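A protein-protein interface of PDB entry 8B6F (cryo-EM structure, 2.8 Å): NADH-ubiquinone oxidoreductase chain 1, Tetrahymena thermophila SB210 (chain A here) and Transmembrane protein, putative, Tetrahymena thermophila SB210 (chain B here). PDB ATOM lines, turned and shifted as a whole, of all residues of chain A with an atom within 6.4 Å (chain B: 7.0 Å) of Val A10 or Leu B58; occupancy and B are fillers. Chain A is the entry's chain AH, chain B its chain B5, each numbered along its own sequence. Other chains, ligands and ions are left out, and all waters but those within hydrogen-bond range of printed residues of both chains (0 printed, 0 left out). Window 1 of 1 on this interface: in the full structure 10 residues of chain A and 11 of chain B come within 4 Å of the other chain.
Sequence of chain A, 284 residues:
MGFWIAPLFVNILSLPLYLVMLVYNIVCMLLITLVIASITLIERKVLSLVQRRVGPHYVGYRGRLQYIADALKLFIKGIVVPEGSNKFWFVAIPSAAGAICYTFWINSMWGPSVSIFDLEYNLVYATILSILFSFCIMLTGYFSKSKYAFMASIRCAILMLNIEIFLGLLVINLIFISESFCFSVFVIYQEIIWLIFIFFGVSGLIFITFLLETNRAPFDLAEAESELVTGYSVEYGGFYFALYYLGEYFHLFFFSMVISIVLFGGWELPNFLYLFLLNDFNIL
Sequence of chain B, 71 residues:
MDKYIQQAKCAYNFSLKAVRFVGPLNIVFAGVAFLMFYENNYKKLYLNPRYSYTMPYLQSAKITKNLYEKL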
ATOM      1  N   ILE A   5     -17.467  11.831  -0.946  1.00  0.00           N
ATOM      2  CA  ILE A   5     -16.360  12.723  -1.275  1.00  0.00           C
ATOM      3  C   ILE A   5     -15.589  12.160  -2.462  1.00  0.00           C
ATOM      4  O   ILE A   5     -14.961  12.910  -3.218  1.00  0.00           O
ATOM      5  CB  ILE A   5     -15.436  12.928  -0.059  1.00  0.00           C
ATOM      6  CG1 ILE A   5     -16.194  13.648   1.060  1.00  0.00           C
ATOM      7  CG2 ILE A   5     -14.192  13.717  -0.451  1.00  0.00           C
ATOM      8  CD1 ILE A   5     -15.442  13.719   2.374  1.00  0.00           C
ATOM      9  N   ALA A   6     -15.634  10.842  -2.635  1.00  0.00           N
ATOM     10  CA  ALA A   6     -14.900  10.222  -3.734  1.00  0.00           C
ATOM     11  C   ALA A   6     -15.259  10.806  -5.093  1.00  0.00           C
ATOM     12  O   ALA A   6     -14.336  11.036  -5.896  1.00  0.00           O
ATOM     13  CB  ALA A   6     -15.136   8.707  -3.719  1.00  0.00           C
ATOM     14  N   PRO A   7     -16.526  11.067  -5.423  1.00  0.00           N
ATOM     15  CA  PRO A   7     -16.832  11.591  -6.764  1.00  0.00           C
ATOM     16  C   PRO A   7     -16.114  12.889  -7.087  1.00  0.00           C
ATOM     17  O   PRO A   7     -15.841  13.157  -8.262  1.00  0.00           O
ATOM     18  CB  PRO A   7     -18.355  11.782  -6.726  1.00  0.00           C
ATOM     19  CG  PRO A   7     -18.830  10.853  -5.668  1.00  0.00           C
ATOM     20  CD  PRO A   7     -17.748  10.828  -4.635  1.00  0.00           C
ATOM     21  N   LEU A   8     -15.804  13.708  -6.081  1.00  0.00           N
ATOM     22  CA  LEU A   8     -15.177  15.000  -6.333  1.00  0.00           C
ATOM     23  C   LEU A   8     -13.764  14.874  -6.889  1.00  0.00           C
ATOM     24  O   LEU A   8     -13.268  15.829  -7.496  1.00  0.00           O
ATOM     25  CB  LEU A   8     -15.144  15.826  -5.046  1.00  0.00           C
ATOM     26  CG  LEU A   8     -16.503  16.213  -4.458  1.00  0.00           C
ATOM     27  CD1 LEU A   8     -16.328  16.867  -3.099  1.00  0.00           C
ATOM     28  CD2 LEU A   8     -17.257  17.137  -5.400  1.00  0.00           C
ATOM     29  N   PHE A   9     -13.107  13.730  -6.700  1.00  0.00           N
ATOM     30  CA  PHE A   9     -11.705  13.564  -7.068  1.00  0.00           C
ATOM     31  C   PHE A   9     -11.503  12.659  -8.278  1.00  0.00           C
ATOM     32  O   PHE A   9     -10.359  12.336  -8.608  1.00  0.00           O
ATOM     33  CB  PHE A   9     -10.914  13.023  -5.876  1.00  0.00           C
ATOM     34  CG  PHE A   9     -10.859  13.968  -4.713  1.00  0.00           C
ATOM     35  CD1 PHE A   9      -9.959  15.021  -4.704  1.00  0.00           C
ATOM     36  CD2 PHE A   9     -11.701  13.803  -3.627  1.00  0.00           C
ATOM     37  CE1 PHE A   9      -9.903  15.893  -3.634  1.00  0.00           C
ATOM     38  CE2 PHE A   9     -11.650  14.672  -2.555  1.00  0.00           C
ATOM     39  CZ  PHE A   9     -10.750  15.718  -2.558  1.00  0.00           C
ATOM     40  N   VAL A  10     -12.578  12.242  -8.948  1.00  0.00           N
ATOM     41  CA  VAL A  10     -12.434  11.322 -10.074  1.00  0.00           C
ATOM     42  C   VAL A  10     -11.535  11.928 -11.145  1.00  0.00           C
ATOM     43  O   VAL A  10     -10.606  11.279 -11.640  1.00  0.00           O
ATOM     44  CB  VAL A  10     -13.815  10.949 -10.644  1.00  0.00           C
ATOM     45  CG1 VAL A  10     -13.669  10.113 -11.907  1.00  0.00           C
ATOM     46  CG2 VAL A  10     -14.633  10.202  -9.606  1.00  0.00           C
ATOM     47  N   ASN A  11     -11.795  13.180 -11.518  1.00  0.00           N
ATOM     48  CA  ASN A  11     -10.977  13.862 -12.511  1.00  0.00           C
ATOM     49  C   ASN A  11      -9.730  14.502 -11.918  1.00  0.00           C
ATOM     50  O   ASN A  11      -8.822  14.863 -12.674  1.00  0.00           O
ATOM     51  CB  ASN A  11     -11.806  14.934 -13.224  1.00  0.00           C
ATOM     52  CG  ASN A  11     -12.998  14.356 -13.960  1.00  0.00           C
ATOM     53  OD1 ASN A  11     -12.996  13.191 -14.352  1.00  0.00           O
ATOM     54  ND2 ASN A  11     -14.025  15.174 -14.154  1.00  0.00           N
ATOM     55  N   ILE A  12      -9.662  14.650 -10.596  1.00  0.00           N
ATOM     56  CA  ILE A  12      -8.492  15.259  -9.970  1.00  0.00           C
ATOM     57  C   ILE A  12      -7.360  14.251  -9.812  1.00  0.00           C
ATOM     58  O   ILE A  12      -6.184  14.633  -9.814  1.00  0.00           O
ATOM     59  CB  ILE A  12      -8.878  15.876  -8.613  1.00  0.00           C
ATOM     60  CG1 ILE A  12      -9.933  16.972  -8.796  1.00  0.00           C
ATOM     61  CG2 ILE A  12      -7.649  16.431  -7.901  1.00  0.00           C
ATOM     62  CD1 ILE A  12      -9.479  18.156  -9.634  1.00  0.00           C
ATOM     63  N   LEU A  13      -7.676  12.967  -9.674  1.00  0.00           N
ATOM     64  CA  LEU A  13      -6.654  11.947  -9.479  1.00  0.00           C
ATOM     65  C   LEU A  13      -6.011  11.487 -10.779  1.00  0.00           C
ATOM     66  O   LEU A  13      -5.109  10.643 -10.738  1.00  0.00           O
ATOM     67  CB  LEU A  13      -7.265  10.744  -8.755  1.00  0.00           C
ATOM     68  CG  LEU A  13      -7.778  11.019  -7.339  1.00  0.00           C
ATOM     69  CD1 LEU A  13      -8.518   9.813  -6.786  1.00  0.00           C
ATOM     70  CD2 LEU A  13      -6.636  11.408  -6.417  1.00  0.00           C
ATOM     71  N   SER A  14      -6.449  12.007 -11.925  1.00  0.00           N
ATOM     72  CA  SER A  14      -5.873  11.653 -13.213  1.00  0.00           C
ATOM     73  C   SER A  14      -4.833  12.643 -13.707  1.00  0.00           C
ATOM     74  O   SER A  14      -4.003  12.277 -14.545  1.00  0.00           O
ATOM     75  CB  SER A  14      -6.971  11.534 -14.266  1.00  0.00           C
ATOM     76  OG  SER A  14      -7.847  10.492 -13.912  1.00  0.00           O
ATOM     77  N   PHE B  37     -21.213  18.161 -12.495  1.00  0.00           N
ATOM     78  CA  PHE B  37     -19.950  17.470 -12.273  1.00  0.00           C
ATOM     79  C   PHE B  37     -20.108  16.358 -11.244  1.00  0.00           C
ATOM     80  O   PHE B  37     -19.672  15.224 -11.463  1.00  0.00           O
ATOM     81  CB  PHE B  37     -18.891  18.482 -11.830  1.00  0.00           C
ATOM     82  CG  PHE B  37     -17.643  17.862 -11.277  1.00  0.00           C
ATOM     83  CD1 PHE B  37     -16.627  17.450 -12.120  1.00  0.00           C
ATOM     84  CD2 PHE B  37     -17.472  17.723  -9.910  1.00  0.00           C
ATOM     85  CE1 PHE B  37     -15.471  16.891 -11.613  1.00  0.00           C
ATOM     86  CE2 PHE B  37     -16.319  17.165  -9.395  1.00  0.00           C
ATOM     87  CZ  PHE B  37     -15.317  16.748 -10.250  1.00  0.00           C
ATOM     88  N   ASN B  40     -22.340  13.441 -12.564  1.00  0.00           N
ATOM     89  CA  ASN B  40     -21.625  12.641 -13.551  1.00  0.00           C
ATOM     90  C   ASN B  40     -20.630  11.704 -12.877  1.00  0.00           C
ATOM     91  O   ASN B  40     -20.609  10.500 -13.154  1.00  0.00           O
ATOM     92  CB  ASN B  40     -20.915  13.564 -14.540  1.00  0.00           C
ATOM     93  CG  ASN B  40     -20.118  12.806 -15.577  1.00  0.00           C
ATOM     94  OD1 ASN B  40     -20.338  11.617 -15.799  1.00  0.00           O
ATOM     95  ND2 ASN B  40     -19.184  13.494 -16.221  1.00  0.00           N
ATOM     96  N   ASN B  41     -19.795  12.241 -11.986  1.00  0.00           N
ATOM     97  CA  ASN B  41     -18.804  11.409 -11.313  1.00  0.00           C
ATOM     98  C   ASN B  41     -19.471  10.347 -10.448  1.00  0.00           C
ATOM     99  O   ASN B  41     -19.016   9.199 -10.398  1.00  0.00           O
ATOM    100  CB  ASN B  41     -17.871  12.277 -10.472  1.00  0.00           C
ATOM    101  CG  ASN B  41     -16.915  13.089 -11.318  1.00  0.00           C
ATOM    102  OD1 ASN B  41     -17.061  13.166 -12.535  1.00  0.00           O
ATOM    103  ND2 ASN B  41     -15.933  13.706 -10.675  1.00  0.00           N
ATOM    104  N   TYR B  42     -20.554  10.711  -9.759  1.00  0.00           N
ATOM    105  CA  TYR B  42     -21.237   9.760  -8.890  1.00  0.00           C
ATOM    106  C   TYR B  42     -21.811   8.598  -9.691  1.00  0.00           C
ATOM    107  O   TYR B  42     -21.664   7.433  -9.309  1.00  0.00           O
ATOM    108  CB  TYR B  42     -22.341  10.477  -8.111  1.00  0.00           C
ATOM    109  CG  TYR B  42     -23.084   9.596  -7.133  1.00  0.00           C
ATOM    110  CD1 TYR B  42     -24.170   8.832  -7.541  1.00  0.00           C
ATOM    111  CD2 TYR B  42     -22.712   9.546  -5.798  1.00  0.00           C
ATOM    112  CE1 TYR B  42     -24.854   8.033  -6.647  1.00  0.00           C
ATOM    113  CE2 TYR B  42     -23.390   8.750  -4.898  1.00  0.00           C
ATOM    114  CZ  TYR B  42     -24.459   7.995  -5.328  1.00  0.00           C
ATOM    115  OH  TYR B  42     -25.138   7.202  -4.436  1.00  0.00           O
ATOM    116  N   LYS B  44     -20.817   7.601 -12.630  1.00  0.00           N
ATOM    117  CA  LYS B  44     -19.715   6.847 -13.209  1.00  0.00           C
ATOM    118  C   LYS B  44     -18.966   6.026 -12.172  1.00  0.00           C
ATOM    119  O   LYS B  44     -18.277   5.069 -12.541  1.00  0.00           O
ATOM    120  CB  LYS B  44     -18.740   7.795 -13.912  1.00  0.00           C
ATOM    121  CG  LYS B  44     -17.633   7.087 -14.685  1.00  0.00           C
ATOM    122  CD  LYS B  44     -16.741   8.081 -15.417  1.00  0.00           C
ATOM    123  CE  LYS B  44     -15.662   7.363 -16.215  1.00  0.00           C
ATOM    124  NZ  LYS B  44     -14.728   8.313 -16.884  1.00  0.00           N
ATOM    125  N   LEU B  45     -19.084   6.371 -10.891  1.00  0.00           N
ATOM    126  CA  LEU B  45     -18.310   5.719  -9.845  1.00  0.00           C
ATOM    127  C   LEU B  45     -19.100   4.695  -9.043  1.00  0.00           C
ATOM    128  O   LEU B  45     -18.500   3.755  -8.513  1.00  0.00           O
ATOM    129  CB  LEU B  45     -17.740   6.774  -8.890  1.00  0.00           C
ATOM    130  CG  LEU B  45     -16.790   6.289  -7.794  1.00  0.00           C
ATOM    131  CD1 LEU B  45     -15.548   5.645  -8.388  1.00  0.00           C
ATOM    132  CD2 LEU B  45     -16.407   7.445  -6.892  1.00  0.00           C
ATOM    133  N   ARG B  50     -17.950  -1.379 -13.506  1.00  0.00           N
ATOM    134  CA  ARG B  50     -16.582  -1.175 -13.035  1.00  0.00           C
ATOM    135  C   ARG B  50     -15.699  -2.389 -13.304  1.00  0.00           C
ATOM    136  O   ARG B  50     -14.761  -2.665 -12.553  1.00  0.00           O
ATOM    137  CB  ARG B  50     -16.562  -0.819 -11.546  1.00  0.00           C
ATOM    138  CG  ARG B  50     -17.204   0.527 -11.243  1.00  0.00           C
ATOM    139  CD  ARG B  50     -17.211   0.833  -9.755  1.00  0.00           C
ATOM    140  NE  ARG B  50     -15.867   0.923  -9.198  1.00  0.00           N
ATOM    141  CZ  ARG B  50     -15.591   1.340  -7.971  1.00  0.00           C
ATOM    142  NH1 ARG B  50     -16.545   1.733  -7.144  1.00  0.00           N
ATOM    143  NH2 ARG B  50     -14.326   1.367  -7.562  1.00  0.00           N
ATOM    144  N   TYR B  53     -10.952  -0.596 -16.048  1.00  0.00           N
ATOM    145  CA  TYR B  53     -10.203   0.373 -15.251  1.00  0.00           C
ATOM    146  C   TYR B  53     -10.343   1.748 -15.888  1.00  0.00           C
ATOM    147  O   TYR B  53      -9.603   2.099 -16.808  1.00  0.00           O
ATOM    148  CB  TYR B  53      -8.742  -0.046 -15.154  1.00  0.00           C
ATOM    149  CG  TYR B  53      -7.978   0.659 -14.061  1.00  0.00           C
ATOM    150  CD1 TYR B  53      -8.011   0.190 -12.757  1.00  0.00           C
ATOM    151  CD2 TYR B  53      -7.218   1.786 -14.335  1.00  0.00           C
ATOM    152  CE1 TYR B  53      -7.314   0.825 -11.754  1.00  0.00           C
ATOM    153  CE2 TYR B  53      -6.518   2.429 -13.339  1.00  0.00           C
ATOM    154  CZ  TYR B  53      -6.570   1.942 -12.052  1.00  0.00           C
ATOM    155  OH  TYR B  53      -5.874   2.580 -11.056  1.00  0.00           O
ATOM    156  N   THR B  54     -11.296   2.537 -15.395  1.00  0.00           N
ATOM    157  CA  THR B  54     -11.585   3.853 -15.950  1.00  0.00           C
ATOM    158  C   THR B  54     -11.208   5.000 -15.029  1.00  0.00           C
ATOM    159  O   THR B  54     -10.824   6.063 -15.520  1.00  0.00           O
ATOM    160  CB  THR B  54     -13.075   3.972 -16.293  1.00  0.00           C
ATOM    161  OG1 THR B  54     -13.487   2.834 -17.061  1.00  0.00           O
ATOM    162  CG2 THR B  54     -13.339   5.235 -17.098  1.00  0.00           C
ATOM    163  N   MET B  55     -11.310   4.821 -13.712  1.00  0.00           N
ATOM    164  CA  MET B  55     -10.956   5.868 -12.759  1.00  0.00           C
ATOM    165  C   MET B  55      -9.728   5.439 -11.969  1.00  0.00           C
ATOM    166  O   MET B  55      -9.845   4.640 -11.027  1.00  0.00           O
ATOM    167  CB  MET B  55     -12.125   6.156 -11.812  1.00  0.00           C
ATOM    168  CG  MET B  55     -13.353   6.733 -12.496  1.00  0.00           C
ATOM    169  SD  MET B  55     -14.443   5.482 -13.192  1.00  0.00           S
ATOM    170  CE  MET B  55     -15.142   4.787 -11.701  1.00  0.00           C
ATOM    171  N   PRO B  56      -8.537   5.933 -12.301  1.00  0.00           N
ATOM    172  CA  PRO B  56      -7.344   5.535 -11.547  1.00  0.00           C
ATOM    173  C   PRO B  56      -7.405   6.033 -10.114  1.00  0.00           C
ATOM    174  O   PRO B  56      -8.026   7.054  -9.812  1.00  0.00           O
ATOM    175  CB  PRO B  56      -6.194   6.193 -12.319  1.00  0.00           C
ATOM    176  CG  PRO B  56      -6.824   7.312 -13.058  1.00  0.00           C
ATOM    177  CD  PRO B  56      -8.210   6.865 -13.394  1.00  0.00           C
ATOM    178  N   TYR B  57      -6.760   5.283  -9.221  1.00  0.00           N
ATOM    179  CA  TYR B  57      -6.640   5.596  -7.801  1.00  0.00           C
ATOM    180  C   TYR B  57      -7.951   5.386  -7.057  1.00  0.00           C
ATOM    181  O   TYR B  57      -7.984   5.542  -5.832  1.00  0.00           O
ATOM    182  CB  TYR B  57      -6.152   7.032  -7.564  1.00  0.00           C
ATOM    183  CG  TYR B  57      -4.756   7.278  -8.086  1.00  0.00           C
ATOM    184  CD1 TYR B  57      -3.641   6.876  -7.362  1.00  0.00           C
ATOM    185  CD2 TYR B  57      -4.556   7.907  -9.307  1.00  0.00           C
ATOM    186  CE1 TYR B  57      -2.365   7.099  -7.841  1.00  0.00           C
ATOM    187  CE2 TYR B  57      -3.287   8.136  -9.793  1.00  0.00           C
ATOM    188  CZ  TYR B  57      -2.196   7.727  -9.058  1.00  0.00           C
ATOM    189  OH  TYR B  57      -0.931   7.955  -9.543  1.00  0.00           O
ATOM    190  N   LEU B  58      -9.027   5.034  -7.753  1.00  0.00           N
ATOM    191  CA  LEU B  58     -10.314   4.703  -7.153  1.00  0.00           C
ATOM    192  C   LEU B  58     -10.707   3.255  -7.379  1.00  0.00           C
ATOM    193  O   LEU B  58     -11.297   2.636  -6.491  1.00  0.00           O
ATOM    194  CB  LEU B  58     -11.404   5.625  -7.718  1.00  0.00           C
ATOM    195  CG  LEU B  58     -11.207   7.119  -7.453  1.00  0.00           C
ATOM    196  CD1 LEU B  58     -12.300   7.928  -8.121  1.00  0.00           C
ATOM    197  CD2 LEU B  58     -11.169   7.415  -5.963  1.00  0.00           C
ATOM    198  N   GLN B  59     -10.397   2.699  -8.545  1.00  0.00           N
ATOM    199  CA  GLN B  59     -10.559   1.275  -8.785  1.00  0.00           C
ATOM    200  C   GLN B  59      -9.253   0.555  -8.481  1.00  0.00           C
ATOM    201  O   GLN B  59      -8.161   1.091  -8.690  1.00  0.00           O
ATOM    202  CB  GLN B  59     -10.972   1.007 -10.233  1.00  0.00           C
ATOM    203  CG  GLN B  59     -12.280   1.656 -10.643  1.00  0.00           C
ATOM    204  CD  GLN B  59     -12.769   1.165 -11.989  1.00  0.00           C
ATOM    205  OE1 GLN B  59     -12.218   0.227 -12.558  1.00  0.00           O
ATOM    206  NE2 GLN B  59     -13.814   1.800 -12.506  1.00  0.00           N
ATOM    207  N   SER B  60      -9.372  -0.670  -7.983  1.00  0.00           N
ATOM    208  CA  SER B  60      -8.192  -1.458  -7.663  1.00  0.00           C
ATOM    209  C   SER B  60      -7.408  -1.784  -8.929  1.00  0.00           C
ATOM    210  O   SER B  60      -7.966  -1.905 -10.021  1.00  0.00           O
ATOM    211  CB  SER B  60      -8.585  -2.749  -6.944  1.00  0.00           C
ATOM    212  OG  SER B  60      -9.403  -3.561  -7.765  1.00  0.00           O
ATOM    213  N   LEU B  71     -13.129  -4.032 -10.210  1.00  0.00           N
ATOM    214  CA  LEU B  71     -11.934  -3.282  -9.849  1.00  0.00           C
ATOM    215  C   LEU B  71     -12.283  -2.118  -8.931  1.00  0.00           C
ATOM    216  O   LEU B  71     -13.408  -1.623  -8.943  1.00  0.00           O
ATOM    217  CB  LEU B  71     -11.225  -2.768 -11.104  1.00  0.00           C
ATOM    218  CG  LEU B  71     -10.786  -3.831 -12.115  1.00  0.00           C
ATOM    219  CD1 LEU B  71     -10.168  -3.178 -13.338  1.00  0.00           C
ATOM    220  CD2 LEU B  71      -9.814  -4.817 -11.489  1.00  0.00           C
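O of Pro A7 sits at hydrogen-bond distance from ND2 of Asn B41 (2.5 Å).
The guanidinium group (NH2) of Arg B50 sits at hydrogen-bond distance from the backbone carbonyl oxygen (O) of Leu B58, at 3.5 Å.
The side-chain amide nitrogen of Gln B59 sits close to the side-chain sulfur of Met B55 (3.8 Å).
The backbone carbonyl oxygen (O) of Phe B37 lies close to the side-chain amide oxygen (OD1) of Asn B41 (3.5 Å).
N of Tyr B57 is in hydrogen-bond range of OH of Tyr B53 (3.4 Å).
The guanidinium group of Arg B50 sits at hydrogen-bond distance from the backbone carbonyl oxygen of Leu B45, 3.1 Å away.
Leu B45 touches Ala A6.
Tyr B42 touches Pro A7.
Pro A7 touches Leu B45 (N to CD2, 3.9 Å).
Leu A8 touches Phe B37 (O to CZ, 3.6 Å).
CB of Val A10 touches ND2 of Asn B41, at 3.5 Å.
Val A10 touches Leu B58.
Asn A11 touches Phe B37.
Asn A11 touches Asn B41 (ND2 to OD1, 3.98 Å).
Pro B56 touches Leu A13 (O to CB, 3.9 Å).
Leu A13 touches Leu B58.
Of the printed residues of chain B, Pro A7 touches Asn B41 (2.5 Å), Tyr B42 (3.9 Å) and Leu B45 (3.9 Å).
Of chain B, only Asn B41 (3.5 Å), Met B55 (3.4 Å) and Leu B58 (3.6 Å) come within 4 Å of Val A10.
Of the printed residues of chain B, Asn A11 touches Phe B37 and Asn B41.
Of the printed residues of chain B, Leu A13 touches Pro B56, Tyr B57 and Leu B58.
Of the 10 printed residues of chain A, 7 touch a printed residue of chain B.
Printed residues of chain A that touch a printed residue of chain B: Ala A6, Pro A7, Leu A8, Val A10, Asn A11, Leu A13 and Ser A14.
Hydrophobic or aromatic side chains of chain A that line the printed part of chain B: Ala A6, Pro A7, Val A10 and Leu A13.
Of the 16 printed residues of chain B, 8 touch a printed residue of chain A.
Printed residues of chain B that touch a printed residue of chain A: Phe B37, Asn B41, Tyr B42, Leu B45, Met B55, Pro B56, Tyr B57 and Leu B58.
Hydrophobic or aromatic side chains of chain B within 4 Å of the printed part of chain A: Phe B37, Leu B45, Met B55, Pro B56, Tyr B57 and Leu B58.
Among the printed residues, 14 pairs touch across the chains.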
